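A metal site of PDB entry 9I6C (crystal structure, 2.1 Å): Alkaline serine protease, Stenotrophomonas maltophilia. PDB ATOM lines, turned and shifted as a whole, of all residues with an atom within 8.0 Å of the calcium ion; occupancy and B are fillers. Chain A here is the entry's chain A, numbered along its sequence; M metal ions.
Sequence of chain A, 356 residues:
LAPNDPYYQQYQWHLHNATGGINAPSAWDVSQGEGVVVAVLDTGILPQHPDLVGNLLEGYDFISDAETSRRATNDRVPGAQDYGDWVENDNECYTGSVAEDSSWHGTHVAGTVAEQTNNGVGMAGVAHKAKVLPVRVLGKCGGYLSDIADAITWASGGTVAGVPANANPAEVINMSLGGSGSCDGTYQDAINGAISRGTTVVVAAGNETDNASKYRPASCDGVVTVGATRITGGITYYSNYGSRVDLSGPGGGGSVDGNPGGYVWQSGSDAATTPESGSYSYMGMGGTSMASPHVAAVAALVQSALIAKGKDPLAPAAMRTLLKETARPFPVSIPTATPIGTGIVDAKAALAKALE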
ATOM      1  N   PRO A   3       6.169  17.010  -9.364  1.00  0.00           N
ATOM      2  CA  PRO A   3       5.709  16.536 -10.672  1.00  0.00           C
ATOM      3  C   PRO A   3       4.609  15.479 -10.548  1.00  0.00           C
ATOM      4  O   PRO A   3       4.484  14.837  -9.481  1.00  0.00           O
ATOM      5  CB  PRO A   3       7.019  15.913 -11.217  1.00  0.00           C
ATOM      6  CG  PRO A   3       7.666  15.326  -9.961  1.00  0.00           C
ATOM      7  CD  PRO A   3       7.529  16.522  -9.014  1.00  0.00           C
ATOM      8  N   ASN A   4       3.916  15.222 -11.672  1.00  0.00           N
ATOM      9  CA  ASN A   4       2.688  14.438 -11.600  1.00  0.00           C
ATOM     10  C   ASN A   4       2.949  12.929 -11.761  1.00  0.00           C
ATOM     11  O   ASN A   4       1.972  12.170 -11.846  1.00  0.00           O
ATOM     12  CB  ASN A   4       1.632  14.902 -12.617  1.00  0.00           C
ATOM     13  CG  ASN A   4       2.132  14.543 -14.010  1.00  0.00           C
ATOM     14  OD1 ASN A   4       3.166  13.855 -14.164  1.00  0.00           O
ATOM     15  ND2 ASN A   4       1.443  15.014 -15.040  1.00  0.00           N
ATOM     16  N   ASP A   5       4.202  12.445 -11.743  1.00  0.00           N
ATOM     17  CA  ASP A   5       4.416  11.026 -11.994  1.00  0.00           C
ATOM     18  C   ASP A   5       3.718  10.161 -10.935  1.00  0.00           C
ATOM     19  O   ASP A   5       3.998  10.294  -9.736  1.00  0.00           O
ATOM     20  CB  ASP A   5       5.900  10.697 -12.049  1.00  0.00           C
ATOM     21  CG  ASP A   5       6.641  11.644 -12.972  1.00  0.00           C
ATOM     22  OD1 ASP A   5       6.903  12.810 -12.576  1.00  0.00           O
ATOM     23  OD2 ASP A   5       6.999  11.195 -14.091  1.00  0.00           O
ATOM     24  N   PRO A   6       2.838   9.185 -11.348  1.00  0.00           N
ATOM     25  CA  PRO A   6       2.050   8.416 -10.373  1.00  0.00           C
ATOM     26  C   PRO A   6       2.771   7.862  -9.133  1.00  0.00           C
ATOM     27  O   PRO A   6       2.211   7.966  -8.046  1.00  0.00           O
ATOM     28  CB  PRO A   6       1.313   7.317 -11.159  1.00  0.00           C
ATOM     29  CG  PRO A   6       1.546   7.665 -12.623  1.00  0.00           C
ATOM     30  CD  PRO A   6       2.633   8.736 -12.753  1.00  0.00           C
ATOM     31  N   TYR A   7       3.974   7.294  -9.275  1.00  0.00           N
ATOM     32  CA  TYR A   7       4.629   6.631  -8.147  1.00  0.00           C
ATOM     33  C   TYR A   7       5.702   7.488  -7.461  1.00  0.00           C
ATOM     34  O   TYR A   7       6.344   7.023  -6.516  1.00  0.00           O
ATOM     35  CB  TYR A   7       5.312   5.354  -8.659  1.00  0.00           C
ATOM     36  CG  TYR A   7       4.402   4.282  -9.233  1.00  0.00           C
ATOM     37  CD1 TYR A   7       3.180   3.985  -8.624  1.00  0.00           C
ATOM     38  CD2 TYR A   7       4.736   3.524 -10.357  1.00  0.00           C
ATOM     39  CE1 TYR A   7       2.347   2.967  -9.070  1.00  0.00           C
ATOM     40  CE2 TYR A   7       3.903   2.517 -10.843  1.00  0.00           C
ATOM     41  CZ  TYR A   7       2.741   2.200 -10.143  1.00  0.00           C
ATOM     42  OH  TYR A   7       1.796   1.316 -10.532  1.00  0.00           O
ATOM     43  N   TYR A   8       5.862   8.743  -7.889  1.00  0.00           N
ATOM     44  CA  TYR A   8       6.875   9.652  -7.353  1.00  0.00           C
ATOM     45  C   TYR A   8       6.684   9.896  -5.865  1.00  0.00           C
ATOM     46  O   TYR A   8       7.585   9.647  -5.083  1.00  0.00           O
ATOM     47  CB  TYR A   8       6.960  10.981  -8.124  1.00  0.00           C
ATOM     48  CG  TYR A   8       7.575  12.190  -7.418  1.00  0.00           C
ATOM     49  CD1 TYR A   8       8.954  12.302  -7.279  1.00  0.00           C
ATOM     50  CD2 TYR A   8       6.788  13.245  -6.933  1.00  0.00           C
ATOM     51  CE1 TYR A   8       9.520  13.436  -6.713  1.00  0.00           C
ATOM     52  CE2 TYR A   8       7.350  14.372  -6.343  1.00  0.00           C
ATOM     53  CZ  TYR A   8       8.718  14.486  -6.244  1.00  0.00           C
ATOM     54  OH  TYR A   8       9.369  15.568  -5.649  1.00  0.00           O
ATOM     55  N   GLN A  12       9.508   7.729  -4.108  1.00  0.00           N
ATOM     56  CA  GLN A  12      10.826   8.293  -4.428  1.00  0.00           C
ATOM     57  C   GLN A  12      11.404   9.197  -3.347  1.00  0.00           C
ATOM     58  O   GLN A  12      11.699  10.364  -3.602  1.00  0.00           O
ATOM     59  CB  GLN A  12      11.026   8.835  -5.834  1.00  0.00           C
ATOM     60  CG  GLN A  12      10.780   7.770  -6.880  1.00  0.00           C
ATOM     61  CD  GLN A  12      10.951   8.322  -8.264  1.00  0.00           C
ATOM     62  OE1 GLN A  12      10.214   9.216  -8.722  1.00  0.00           O
ATOM     63  NE2 GLN A  12      11.979   7.837  -8.911  1.00  0.00           N
ATOM     64  N   HIS A  49      11.908   1.612 -23.182  1.00  0.00           N
ATOM     65  CA  HIS A  49      11.127   1.813 -21.954  1.00  0.00           C
ATOM     66  C   HIS A  49      10.331   3.114 -22.091  1.00  0.00           C
ATOM     67  O   HIS A  49      10.895   4.141 -22.461  1.00  0.00           O
ATOM     68  CB  HIS A  49      12.015   1.976 -20.703  1.00  0.00           C
ATOM     69  CG  HIS A  49      11.260   1.784 -19.444  1.00  0.00           C
ATOM     70  ND1 HIS A  49      10.328   2.713 -19.009  1.00  0.00           N
ATOM     71  CD2 HIS A  49      11.242   0.740 -18.520  1.00  0.00           C
ATOM     72  CE1 HIS A  49       9.790   2.304 -17.834  1.00  0.00           C
ATOM     73  NE2 HIS A  49      10.304   1.095 -17.529  1.00  0.00           N
ATOM     74  N   PRO A  50       8.989   3.103 -21.898  1.00  0.00           N
ATOM     75  CA  PRO A  50       8.203   4.283 -22.212  1.00  0.00           C
ATOM     76  C   PRO A  50       8.453   5.467 -21.268  1.00  0.00           C
ATOM     77  O   PRO A  50       8.028   6.558 -21.572  1.00  0.00           O
ATOM     78  CB  PRO A  50       6.741   3.713 -22.133  1.00  0.00           C
ATOM     79  CG  PRO A  50       6.849   2.628 -21.108  1.00  0.00           C
ATOM     80  CD  PRO A  50       8.170   1.958 -21.447  1.00  0.00           C
ATOM     81  N   ASP A  51       9.141   5.270 -20.126  1.00  0.00           N
ATOM     82  CA  ASP A  51       9.413   6.386 -19.221  1.00  0.00           C
ATOM     83  C   ASP A  51      10.832   6.918 -19.433  1.00  0.00           C
ATOM     84  O   ASP A  51      11.275   7.792 -18.666  1.00  0.00           O
ATOM     85  CB  ASP A  51       9.215   6.064 -17.741  1.00  0.00           C
ATOM     86  CG  ASP A  51       8.678   7.233 -16.924  1.00  0.00           C
ATOM     87  OD1 ASP A  51       8.081   8.126 -17.525  1.00  0.00           O
ATOM     88  OD2 ASP A  51       8.842   7.263 -15.679  1.00  0.00           O
ATOM     89  N   LEU A  52      11.550   6.331 -20.419  1.00  0.00           N
ATOM     90  CA  LEU A  52      12.900   6.757 -20.730  1.00  0.00           C
ATOM     91  C   LEU A  52      13.023   7.309 -22.146  1.00  0.00           C
ATOM     92  O   LEU A  52      13.847   8.193 -22.409  1.00  0.00           O
ATOM     93  CB  LEU A  52      13.812   5.540 -20.649  1.00  0.00           C
ATOM     94  CG  LEU A  52      14.255   5.135 -19.254  1.00  0.00           C
ATOM     95  CD1 LEU A  52      15.514   4.284 -19.444  1.00  0.00           C
ATOM     96  CD2 LEU A  52      14.560   6.350 -18.358  1.00  0.00           C
ATOM     97  N   ALA A 114      17.876  10.555 -15.639  1.00  0.00           N
ATOM     98  CA  ALA A 114      17.052  11.278 -16.621  1.00  0.00           C
ATOM     99  C   ALA A 114      15.728  10.609 -16.950  1.00  0.00           C
ATOM    100  O   ALA A 114      15.194  10.839 -18.047  1.00  0.00           O
ATOM    101  CB  ALA A 114      17.828  11.530 -17.950  1.00  0.00           C
ATOM    102  N   GLU A 115      15.173   9.805 -16.032  1.00  0.00           N
ATOM    103  CA  GLU A 115      13.818   9.299 -16.242  1.00  0.00           C
ATOM    104  C   GLU A 115      12.860  10.446 -16.560  1.00  0.00           C
ATOM    105  O   GLU A 115      12.891  11.463 -15.870  1.00  0.00           O
ATOM    106  CB  GLU A 115      13.340   8.427 -15.079  1.00  0.00           C
ATOM    107  CG  GLU A 115      11.959   7.863 -15.369  1.00  0.00           C
ATOM    108  CD  GLU A 115      11.734   6.573 -14.539  1.00  0.00           C
ATOM    109  OE1 GLU A 115      12.708   6.191 -13.793  1.00  0.00           O
ATOM    110  OE2 GLU A 115      10.572   5.983 -14.662  1.00  0.00           O
ATOM    111  N   GLN A 116      12.044  10.324 -17.636  1.00  0.00           N
ATOM    112  CA  GLN A 116      11.061  11.363 -17.984  1.00  0.00           C
ATOM    113  C   GLN A 116      10.139  11.663 -16.785  1.00  0.00           C
ATOM    114  O   GLN A 116       9.653  10.757 -16.096  1.00  0.00           O
ATOM    115  CB  GLN A 116      10.256  10.912 -19.188  1.00  0.00           C
ATOM    116  CG  GLN A 116      11.167  10.695 -20.401  1.00  0.00           C
ATOM    117  CD  GLN A 116      11.149  11.936 -21.253  1.00  0.00           C
ATOM    118  OE1 GLN A 116      11.074  13.075 -20.753  1.00  0.00           O
ATOM    119  NE2 GLN A 116      11.131  11.714 -22.565  1.00  0.00           N
ATOM    120  N   THR A 117       9.895  12.968 -16.572  1.00  0.00           N
ATOM    121  CA  THR A 117       9.330  13.456 -15.340  1.00  0.00           C
ATOM    122  C   THR A 117       8.191  14.434 -15.660  1.00  0.00           C
ATOM    123  O   THR A 117       8.165  15.105 -16.697  1.00  0.00           O
ATOM    124  CB  THR A 117      10.442  14.158 -14.529  1.00  0.00           C
ATOM    125  OG1 THR A 117      11.393  13.154 -14.195  1.00  0.00           O
ATOM    126  CG2 THR A 117       9.916  14.835 -13.275  1.00  0.00           C
ATOM    127  N   ASN A 118       7.216  14.472 -14.765  1.00  0.00           N
ATOM    128  CA  ASN A 118       6.057  15.309 -14.966  1.00  0.00           C
ATOM    129  C   ASN A 118       5.320  14.887 -16.252  1.00  0.00           C
ATOM    130  O   ASN A 118       4.674  15.729 -16.866  1.00  0.00           O
ATOM    131  CB  ASN A 118       6.411  16.778 -14.735  1.00  0.00           C
ATOM    132  CG  ASN A 118       5.156  17.574 -14.479  1.00  0.00           C
ATOM    133  OD1 ASN A 118       5.026  18.663 -14.999  1.00  0.00           O
ATOM    134  ND2 ASN A 118       4.231  17.084 -13.693  1.00  0.00           N
ATOM    135  N   ASN A 119       5.420  13.598 -16.653  1.00  0.00           N
ATOM    136  CA  ASN A 119       4.816  13.086 -17.869  1.00  0.00           C
ATOM    137  C   ASN A 119       3.628  12.149 -17.568  1.00  0.00           C
ATOM    138  O   ASN A 119       3.145  11.482 -18.466  1.00  0.00           O
ATOM    139  CB  ASN A 119       5.819  12.400 -18.806  1.00  0.00           C
ATOM    140  CG  ASN A 119       6.373  11.112 -18.268  1.00  0.00           C
ATOM    141  OD1 ASN A 119       6.482  10.868 -17.042  1.00  0.00           O
ATOM    142  ND2 ASN A 119       6.813  10.266 -19.187  1.00  0.00           N
ATOM    143  N   GLY A 120       3.125  12.111 -16.333  1.00  0.00           N
ATOM    144  CA  GLY A 120       1.927  11.276 -16.110  1.00  0.00           C
ATOM    145  C   GLY A 120       2.202   9.755 -16.192  1.00  0.00           C
ATOM    146  O   GLY A 120       1.255   8.983 -16.342  1.00  0.00           O
ATOM    147  N   VAL A 121       3.475   9.323 -16.130  1.00  0.00           N
ATOM    148  CA  VAL A 121       3.824   7.917 -16.307  1.00  0.00           C
ATOM    149  C   VAL A 121       4.855   7.533 -15.246  1.00  0.00           C
ATOM    150  O   VAL A 121       5.920   8.111 -15.176  1.00  0.00           O
ATOM    151  CB  VAL A 121       4.385   7.615 -17.731  1.00  0.00           C
ATOM    152  CG1 VAL A 121       4.939   6.196 -17.850  1.00  0.00           C
ATOM    153  CG2 VAL A 121       3.362   7.832 -18.832  1.00  0.00           C
ATOM    154  N   GLY A 122       4.647   6.483 -14.461  1.00  0.00           N
ATOM    155  CA  GLY A 122       5.770   5.898 -13.713  1.00  0.00           C
ATOM    156  C   GLY A 122       6.404   6.782 -12.630  1.00  0.00           C
ATOM    157  O   GLY A 122       5.774   7.158 -11.628  1.00  0.00           O
ATOM    158  N   MET A 123       7.737   7.002 -12.748  1.00  0.00           N
ATOM    159  CA  MET A 123       8.529   7.620 -11.697  1.00  0.00           C
ATOM    160  C   MET A 123       9.181   8.881 -12.283  1.00  0.00           C
ATOM    161  O   MET A 123       9.096   9.130 -13.483  1.00  0.00           O
ATOM    162  CB  MET A 123       9.724   6.738 -11.308  1.00  0.00           C
ATOM    163  CG  MET A 123       9.474   5.244 -10.944  1.00  0.00           C
ATOM    164  SD  MET A 123       9.115   5.156  -9.189  1.00  0.00           S
ATOM    165  CE  MET A 123       8.477   3.498  -8.832  1.00  0.00           C
ATOM    166  N   ALA A 124       9.976   9.614 -11.481  1.00  0.00           N
ATOM    167  CA  ALA A 124      10.722  10.798 -11.912  1.00  0.00           C
ATOM    168  C   ALA A 124      12.212  10.483 -11.984  1.00  0.00           C
ATOM    169  O   ALA A 124      12.673   9.420 -11.487  1.00  0.00           O
ATOM    170  CB  ALA A 124      10.437  11.916 -10.893  1.00  0.00           C
ATOM    171  N   GLY A 125      12.981  11.386 -12.595  1.00  0.00           N
ATOM    172  CA  GLY A 125      14.434  11.354 -12.556  1.00  0.00           C
ATOM    173  C   GLY A 125      14.983  12.749 -12.217  1.00  0.00           C
ATOM    174  O   GLY A 125      14.270  13.772 -12.317  1.00  0.00           O
ATOM    175  N   HIS A 128      16.121  15.521 -15.639  1.00  0.00           N
ATOM    176  CA  HIS A 128      15.118  14.949 -16.520  1.00  0.00           C
ATOM    177  C   HIS A 128      14.986  15.696 -17.854  1.00  0.00           C
ATOM    178  O   HIS A 128      14.151  15.266 -18.699  1.00  0.00           O
ATOM    179  CB  HIS A 128      13.800  14.614 -15.787  1.00  0.00           C
ATOM    180  CG  HIS A 128      13.247  15.808 -15.046  1.00  0.00           C
ATOM    181  ND1 HIS A 128      12.614  16.887 -15.669  1.00  0.00           N
ATOM    182  CD2 HIS A 128      13.253  16.064 -13.730  1.00  0.00           C
ATOM    183  CE1 HIS A 128      12.246  17.759 -14.711  1.00  0.00           C
ATOM    184  NE2 HIS A 128      12.624  17.275 -13.532  1.00  0.00           N
ATOM    185  N   TYR A 282       8.834  -0.828 -13.012  1.00  0.00           N
ATOM    186  CA  TYR A 282       9.602   0.031 -12.119  1.00  0.00           C
ATOM    187  C   TYR A 282      10.143  -0.863 -11.018  1.00  0.00           C
ATOM    188  O   TYR A 282       9.368  -1.615 -10.444  1.00  0.00           O
ATOM    189  CB  TYR A 282       8.743   1.206 -11.632  1.00  0.00           C
ATOM    190  CG  TYR A 282       8.143   1.954 -12.813  1.00  0.00           C
ATOM    191  CD1 TYR A 282       8.866   2.937 -13.504  1.00  0.00           C
ATOM    192  CD2 TYR A 282       6.901   1.536 -13.340  1.00  0.00           C
ATOM    193  CE1 TYR A 282       8.319   3.555 -14.637  1.00  0.00           C
ATOM    194  CE2 TYR A 282       6.378   2.106 -14.502  1.00  0.00           C
ATOM    195  CZ  TYR A 282       7.096   3.106 -15.146  1.00  0.00           C
ATOM    196  OH  TYR A 282       6.602   3.655 -16.318  1.00  0.00           O
HETATM  197 CA    CA M   1       7.775   9.503 -15.462  1.00  0.00          CA
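The side-chain carboxylate (OD1) of Asp 5 sits at hydrogen-bond distance from the backbone NH (N) of Asn 118 (2.8 Å).
The side-chain amide oxygen (OD1) of Asn 4 is in hydrogen-bond range of the backbone NH (N) of Asn 119 (3.4 Å).
The backbone NH of Asp 51 is in hydrogen-bond range of a ring nitrogen (ND1) of His 49, at 3.0 Å.
Six residues have an atom within 4 Å of the calcium ion: Asp 5, Asp 51, Gln 116, Asn 119, Val 121 and Met 123.
Along chain A the residues within 4 Å of the calcium ion span positions 5 to 123.
The calcium ion is bound by the side-chain carboxylate (OD2) of Asp 5, the backbone carbonyl oxygen (O) of Val 121, the backbone carbonyl oxygen (O) of Gln 116, the backbone carbonyl oxygen (O) of Met 123, the side-chain amide oxygen (OD1) of Asn 119, the side-chain carboxylate (OD2) of Asp 51 and the side-chain carboxylate (OD1) of Asp 51.
The calcium ion has seven donor atoms within binding distance.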
